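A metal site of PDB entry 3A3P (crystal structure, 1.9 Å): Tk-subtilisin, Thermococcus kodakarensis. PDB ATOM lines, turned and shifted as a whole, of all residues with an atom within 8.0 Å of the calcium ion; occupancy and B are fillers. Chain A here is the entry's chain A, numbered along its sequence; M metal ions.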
ATOM      1  N   GLN A  12      12.232  -3.451  16.159  1.00  0.00           N
ATOM      2  CA  GLN A  12      13.594  -3.081  16.725  1.00  0.00           C
ATOM      3  C   GLN A  12      13.765  -3.474  18.191  1.00  0.00           C
ATOM      4  O   GLN A  12      12.881  -3.214  18.998  1.00  0.00           O
ATOM      5  CB  GLN A  12      13.864  -1.579  16.565  1.00  0.00           C
ATOM      6  CG  GLN A  12      14.026  -1.129  15.122  1.00  0.00           C
ATOM      7  CD  GLN A  12      15.348  -1.585  14.542  1.00  0.00           C
ATOM      8  OE1 GLN A  12      16.405  -1.461  15.181  1.00  0.00           O
ATOM      9  NE2 GLN A  12      15.300  -2.107  13.331  1.00  0.00           N
ATOM     10  N   PRO A  13      14.917  -4.087  18.529  1.00  0.00           N
ATOM     11  CA  PRO A  13      15.207  -4.465  19.923  1.00  0.00           C
ATOM     12  C   PRO A  13      15.526  -3.233  20.786  1.00  0.00           C
ATOM     13  O   PRO A  13      16.044  -2.248  20.261  1.00  0.00           O
ATOM     14  CB  PRO A  13      16.442  -5.374  19.802  1.00  0.00           C
ATOM     15  CG  PRO A  13      17.121  -4.899  18.560  1.00  0.00           C
ATOM     16  CD  PRO A  13      16.004  -4.476  17.615  1.00  0.00           C
ATOM     17  N   ALA A  14      15.217  -3.279  22.092  1.00  0.00           N
ATOM     18  CA  ALA A  14      15.643  -2.251  23.034  1.00  0.00           C
ATOM     19  C   ALA A  14      17.174  -2.065  23.003  1.00  0.00           C
ATOM     20  O   ALA A  14      17.891  -3.011  22.748  1.00  0.00           O
ATOM     21  CB  ALA A  14      15.206  -2.642  24.461  1.00  0.00           C
ATOM     22  N   GLN A  15      17.646  -0.861  23.291  1.00  0.00           N
ATOM     23  CA  GLN A  15      19.066  -0.547  23.141  1.00  0.00           C
ATOM     24  C   GLN A  15      19.932  -1.229  24.182  1.00  0.00           C
ATOM     25  O   GLN A  15      19.552  -1.247  25.355  1.00  0.00           O
ATOM     26  CB  GLN A  15      19.296   0.961  23.170  1.00  0.00           C
ATOM     27  CG  GLN A  15      20.787   1.352  23.113  1.00  0.00           C
ATOM     28  CD  GLN A  15      20.990   2.829  22.960  1.00  0.00           C
ATOM     29  OE1 GLN A  15      20.858   3.370  21.861  1.00  0.00           O
ATOM     30  NE2 GLN A  15      21.319   3.498  24.054  1.00  0.00           N
ATOM     31  N   THR A  16      21.061  -1.790  23.753  1.00  0.00           N
ATOM     32  CA  THR A  16      22.164  -2.150  24.657  1.00  0.00           C
ATOM     33  C   THR A  16      23.437  -1.426  24.341  1.00  0.00           C
ATOM     34  O   THR A  16      23.638  -1.001  23.199  1.00  0.00           O
ATOM     35  CB  THR A  16      22.696  -3.619  24.530  1.00  0.00           C
ATOM     36  OG1 THR A  16      22.328  -4.236  23.275  1.00  0.00           O
ATOM     37  CG2 THR A  16      22.366  -4.419  25.691  1.00  0.00           C
ATOM     38  N   HIS A  53      19.157   2.446   7.893  1.00  0.00           N
ATOM     39  CA  HIS A  53      19.114   1.765   9.171  1.00  0.00           C
ATOM     40  C   HIS A  53      18.605   2.711  10.249  1.00  0.00           C
ATOM     41  O   HIS A  53      19.185   3.769  10.463  1.00  0.00           O
ATOM     42  CB  HIS A  53      20.497   1.193   9.585  1.00  0.00           C
ATOM     43  CG  HIS A  53      20.408   0.256  10.751  1.00  0.00           C
ATOM     44  ND1 HIS A  53      20.751  -1.078  10.683  1.00  0.00           N
ATOM     45  CD2 HIS A  53      19.971   0.453  12.020  1.00  0.00           C
ATOM     46  CE1 HIS A  53      20.571  -1.652  11.859  1.00  0.00           C
ATOM     47  NE2 HIS A  53      20.087  -0.752  12.685  1.00  0.00           N
ATOM     48  N   PRO A  54      17.540   2.315  10.978  1.00  0.00           N
ATOM     49  CA  PRO A  54      16.976   3.171  12.010  1.00  0.00           C
ATOM     50  C   PRO A  54      18.006   3.625  13.068  1.00  0.00           C
ATOM     51  O   PRO A  54      17.853   4.705  13.663  1.00  0.00           O
ATOM     52  CB  PRO A  54      15.892   2.293  12.650  1.00  0.00           C
ATOM     53  CG  PRO A  54      15.485   1.304  11.593  1.00  0.00           C
ATOM     54  CD  PRO A  54      16.803   1.036  10.840  1.00  0.00           C
ATOM     55  N   ASP A  55      19.055   2.851  13.294  1.00  0.00           N
ATOM     56  CA  ASP A  55      20.019   3.212  14.340  1.00  0.00           C
ATOM     57  C   ASP A  55      21.256   3.923  13.807  1.00  0.00           C
ATOM     58  O   ASP A  55      22.225   4.170  14.551  1.00  0.00           O
ATOM     59  CB  ASP A  55      20.408   1.967  15.165  1.00  0.00           C
ATOM     60  CG  ASP A  55      20.589   2.279  16.633  1.00  0.00           C
ATOM     61  OD1 ASP A  55      19.974   3.247  17.130  1.00  0.00           O
ATOM     62  OD2 ASP A  55      21.337   1.564  17.314  1.00  0.00           O
ATOM     63  N   LEU A  56      21.213   4.247  12.513  1.00  0.00           N
ATOM     64  CA  LEU A  56      22.319   4.906  11.819  1.00  0.00           C
ATOM     65  C   LEU A  56      21.929   6.148  11.032  1.00  0.00           C
ATOM     66  O   LEU A  56      22.736   7.085  10.903  1.00  0.00           O
ATOM     67  CB  LEU A  56      22.976   3.936  10.832  1.00  0.00           C
ATOM     68  CG  LEU A  56      23.638   2.643  11.319  1.00  0.00           C
ATOM     69  CD1 LEU A  56      24.326   2.049  10.093  1.00  0.00           C
ATOM     70  CD2 LEU A  56      24.669   2.906  12.430  1.00  0.00           C
ATOM     71  N   ALA A  93      29.201   5.095  15.380  1.00  0.00           N
ATOM     72  CA  ALA A  93      28.176   6.153  15.375  1.00  0.00           C
ATOM     73  C   ALA A  93      26.729   5.692  15.474  1.00  0.00           C
ATOM     74  O   ALA A  93      25.832   6.476  15.140  1.00  0.00           O
ATOM     75  CB  ALA A  93      28.346   7.071  14.146  1.00  0.00           C
ATOM     76  N   ALA A  94      26.475   4.463  15.943  1.00  0.00           N
ATOM     77  CA  ALA A  94      25.058   4.077  16.197  1.00  0.00           C
ATOM     78  C   ALA A  94      24.463   5.038  17.218  1.00  0.00           C
ATOM     79  O   ALA A  94      25.125   5.417  18.158  1.00  0.00           O
ATOM     80  CB  ALA A  94      24.924   2.614  16.694  1.00  0.00           C
ATOM     81  N   LEU A  95      23.228   5.455  16.997  1.00  0.00           N
ATOM     82  CA  LEU A  95      22.624   6.543  17.749  1.00  0.00           C
ATOM     83  C   LEU A  95      22.318   6.101  19.183  1.00  0.00           C
ATOM     84  O   LEU A  95      22.035   4.920  19.424  1.00  0.00           O
ATOM     85  CB  LEU A  95      21.332   6.948  17.017  1.00  0.00           C
ATOM     86  CG  LEU A  95      21.583   7.641  15.682  1.00  0.00           C
ATOM     87  CD1 LEU A  95      20.428   7.401  14.667  1.00  0.00           C
ATOM     88  CD2 LEU A  95      21.817   9.106  15.917  1.00  0.00           C
ATOM     89  N   ASN A  96      22.373   7.039  20.112  1.00  0.00           N
ATOM     90  CA  ASN A  96      22.022   6.792  21.501  1.00  0.00           C
ATOM     91  C   ASN A  96      20.541   7.130  21.629  1.00  0.00           C
ATOM     92  O   ASN A  96      20.175   8.296  21.696  1.00  0.00           O
ATOM     93  CB  ASN A  96      22.841   7.691  22.403  1.00  0.00           C
ATOM     94  CG  ASN A  96      22.703   7.366  23.897  1.00  0.00           C
ATOM     95  OD1 ASN A  96      21.993   6.448  24.282  1.00  0.00           O
ATOM     96  ND2 ASN A  96      23.392   8.111  24.710  1.00  0.00           N
ATOM     97  N   ASN A  97      19.712   6.101  21.640  1.00  0.00           N
ATOM     98  CA  ASN A  97      18.244   6.256  21.558  1.00  0.00           C
ATOM     99  C   ASN A  97      17.613   5.073  22.290  1.00  0.00           C
ATOM    100  O   ASN A  97      18.223   4.530  23.212  1.00  0.00           O
ATOM    101  CB  ASN A  97      17.767   6.338  20.085  1.00  0.00           C
ATOM    102  CG  ASN A  97      18.290   5.181  19.208  1.00  0.00           C
ATOM    103  OD1 ASN A  97      18.695   4.139  19.701  1.00  0.00           O
ATOM    104  ND2 ASN A  97      18.245   5.365  17.889  1.00  0.00           N
ATOM    105  N   ASP A  98      16.444   4.624  21.860  1.00  0.00           N
ATOM    106  CA  ASP A  98      15.835   3.487  22.535  1.00  0.00           C
ATOM    107  C   ASP A  98      15.981   2.119  21.894  1.00  0.00           C
ATOM    108  O   ASP A  98      15.421   1.142  22.391  1.00  0.00           O
ATOM    109  CB  ASP A  98      14.394   3.817  22.930  1.00  0.00           C
ATOM    110  CG  ASP A  98      14.340   4.956  23.949  1.00  0.00           C
ATOM    111  OD1 ASP A  98      14.682   4.734  25.157  1.00  0.00           O
ATOM    112  OD2 ASP A  98      14.010   6.107  23.543  1.00  0.00           O
ATOM    113  N   ILE A  99      16.759   2.024  20.802  1.00  0.00           N
ATOM    114  CA  ILE A  99      16.875   0.781  20.055  1.00  0.00           C
ATOM    115  C   ILE A  99      18.332   0.351  19.783  1.00  0.00           C
ATOM    116  O   ILE A  99      19.262   1.153  19.828  1.00  0.00           O
ATOM    117  CB  ILE A  99      16.153   0.909  18.665  1.00  0.00           C
ATOM    118  CG1 ILE A  99      16.714   2.110  17.892  1.00  0.00           C
ATOM    119  CG2 ILE A  99      14.612   1.133  18.857  1.00  0.00           C
ATOM    120  CD1 ILE A  99      16.504   2.052  16.409  1.00  0.00           C
ATOM    121  N   GLY A 100      18.500  -0.914  19.457  1.00  0.00           N
ATOM    122  CA  GLY A 100      19.726  -1.399  18.843  1.00  0.00           C
ATOM    123  C   GLY A 100      20.947  -1.282  19.723  1.00  0.00           C
ATOM    124  O   GLY A 100      21.012  -1.839  20.826  1.00  0.00           O
ATOM    125  N   VAL A 101      21.965  -0.614  19.202  1.00  0.00           N
ATOM    126  CA  VAL A 101      23.210  -0.467  19.951  1.00  0.00           C
ATOM    127  C   VAL A 101      23.542   1.011  20.146  1.00  0.00           C
ATOM    128  O   VAL A 101      22.645   1.867  20.057  1.00  0.00           O
ATOM    129  CB  VAL A 101      24.355  -1.239  19.258  1.00  0.00           C
ATOM    130  CG1 VAL A 101      24.084  -2.759  19.321  1.00  0.00           C
ATOM    131  CG2 VAL A 101      24.533  -0.765  17.805  1.00  0.00           C
ATOM    132  N   VAL A 102      24.806   1.357  20.424  1.00  0.00           N
ATOM    133  CA  VAL A 102      25.204   2.772  20.530  1.00  0.00           C
ATOM    134  C   VAL A 102      26.685   2.817  20.162  1.00  0.00           C
ATOM    135  O   VAL A 102      27.437   1.911  20.527  1.00  0.00           O
ATOM    136  CB  VAL A 102      24.885   3.426  21.931  1.00  0.00           C
ATOM    137  CG1 VAL A 102      25.506   2.654  23.125  1.00  0.00           C
ATOM    138  CG2 VAL A 102      25.298   4.916  22.009  1.00  0.00           C
ATOM    139  N   GLY A 103      27.090   3.829  19.373  1.00  0.00           N
ATOM    140  CA  GLY A 103      28.488   3.861  18.966  1.00  0.00           C
ATOM    141  C   GLY A 103      29.344   4.555  20.000  1.00  0.00           C
ATOM    142  O   GLY A 103      28.815   5.117  20.954  1.00  0.00           O
ATOM    143  N   PRO A 106      28.180   8.567  19.479  1.00  0.00           N
ATOM    144  CA  PRO A 106      26.846   8.349  18.927  1.00  0.00           C
ATOM    145  C   PRO A 106      26.180   9.573  18.241  1.00  0.00           C
ATOM    146  O   PRO A 106      25.080   9.423  17.665  1.00  0.00           O
ATOM    147  CB  PRO A 106      26.033   7.880  20.163  1.00  0.00           C
ATOM    148  CG  PRO A 106      26.737   8.367  21.326  1.00  0.00           C
ATOM    149  CD  PRO A 106      28.206   8.529  20.957  1.00  0.00           C
ATOM    150  N   THR A 242      25.383  -2.776  14.249  1.00  0.00           N
ATOM    151  CA  THR A 242      24.374  -2.755  13.203  1.00  0.00           C
ATOM    152  C   THR A 242      24.778  -3.621  12.011  1.00  0.00           C
ATOM    153  O   THR A 242      25.965  -3.827  11.711  1.00  0.00           O
ATOM    154  CB  THR A 242      24.140  -1.305  12.730  1.00  0.00           C
ATOM    155  OG1 THR A 242      25.422  -0.653  12.567  1.00  0.00           O
ATOM    156  CG2 THR A 242      23.323  -0.517  13.780  1.00  0.00           C
ATOM    157  N   TYR A 248      21.115  -6.392  13.346  1.00  0.00           N
ATOM    158  CA  TYR A 248      22.338  -6.383  14.195  1.00  0.00           C
ATOM    159  C   TYR A 248      23.025  -7.739  14.068  1.00  0.00           C
ATOM    160  O   TYR A 248      22.366  -8.738  13.821  1.00  0.00           O
ATOM    161  CB  TYR A 248      21.973  -6.078  15.659  1.00  0.00           C
ATOM    162  CG  TYR A 248      21.132  -4.844  15.744  1.00  0.00           C
ATOM    163  CD1 TYR A 248      19.735  -4.909  15.585  1.00  0.00           C
ATOM    164  CD2 TYR A 248      21.725  -3.606  15.890  1.00  0.00           C
ATOM    165  CE1 TYR A 248      18.965  -3.756  15.594  1.00  0.00           C
ATOM    166  CE2 TYR A 248      20.974  -2.454  15.905  1.00  0.00           C
ATOM    167  CZ  TYR A 248      19.587  -2.533  15.746  1.00  0.00           C
ATOM    168  OH  TYR A 248      18.859  -1.352  15.762  1.00  0.00           O
HETATM  169 CA    CA M   1      20.725   2.972  19.440  1.00  0.00          CA
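The side-chain amide nitrogen (NE2) of Gln 15 sits at hydrogen-bond distance from the side-chain amide oxygen (OD1) of Asn 96 (3.0 Å).
The backbone NH (N) of Gln 15 lies within hydrogen-bond range of the backbone carbonyl oxygen (O) of Asp 98 (3.1 Å).
The nearest printed residue that does not touch the calcium ion is Gly 100 (4.3 Å).
O of Val 101 binds the calcium ion, 2.3 Å away.
The backbone carbonyl oxygen (O) of Leu 95 is bound to the calcium ion, 2.3 Å away.
The calcium ion is bound by OD1 of Asn 97, 2.4 Å away.
The backbone carbonyl oxygen (O) of Ile 99 binds the calcium ion, at 2.4 Å.
The calcium ion is bound by OD1 of Asp 55 (2.4 Å).
OE1 of Gln 15 binds the calcium ion, at 2.5 Å.
OD2 of Asp 55 binds the calcium ion.
The calcium ion has seven donor atoms within binding distance.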
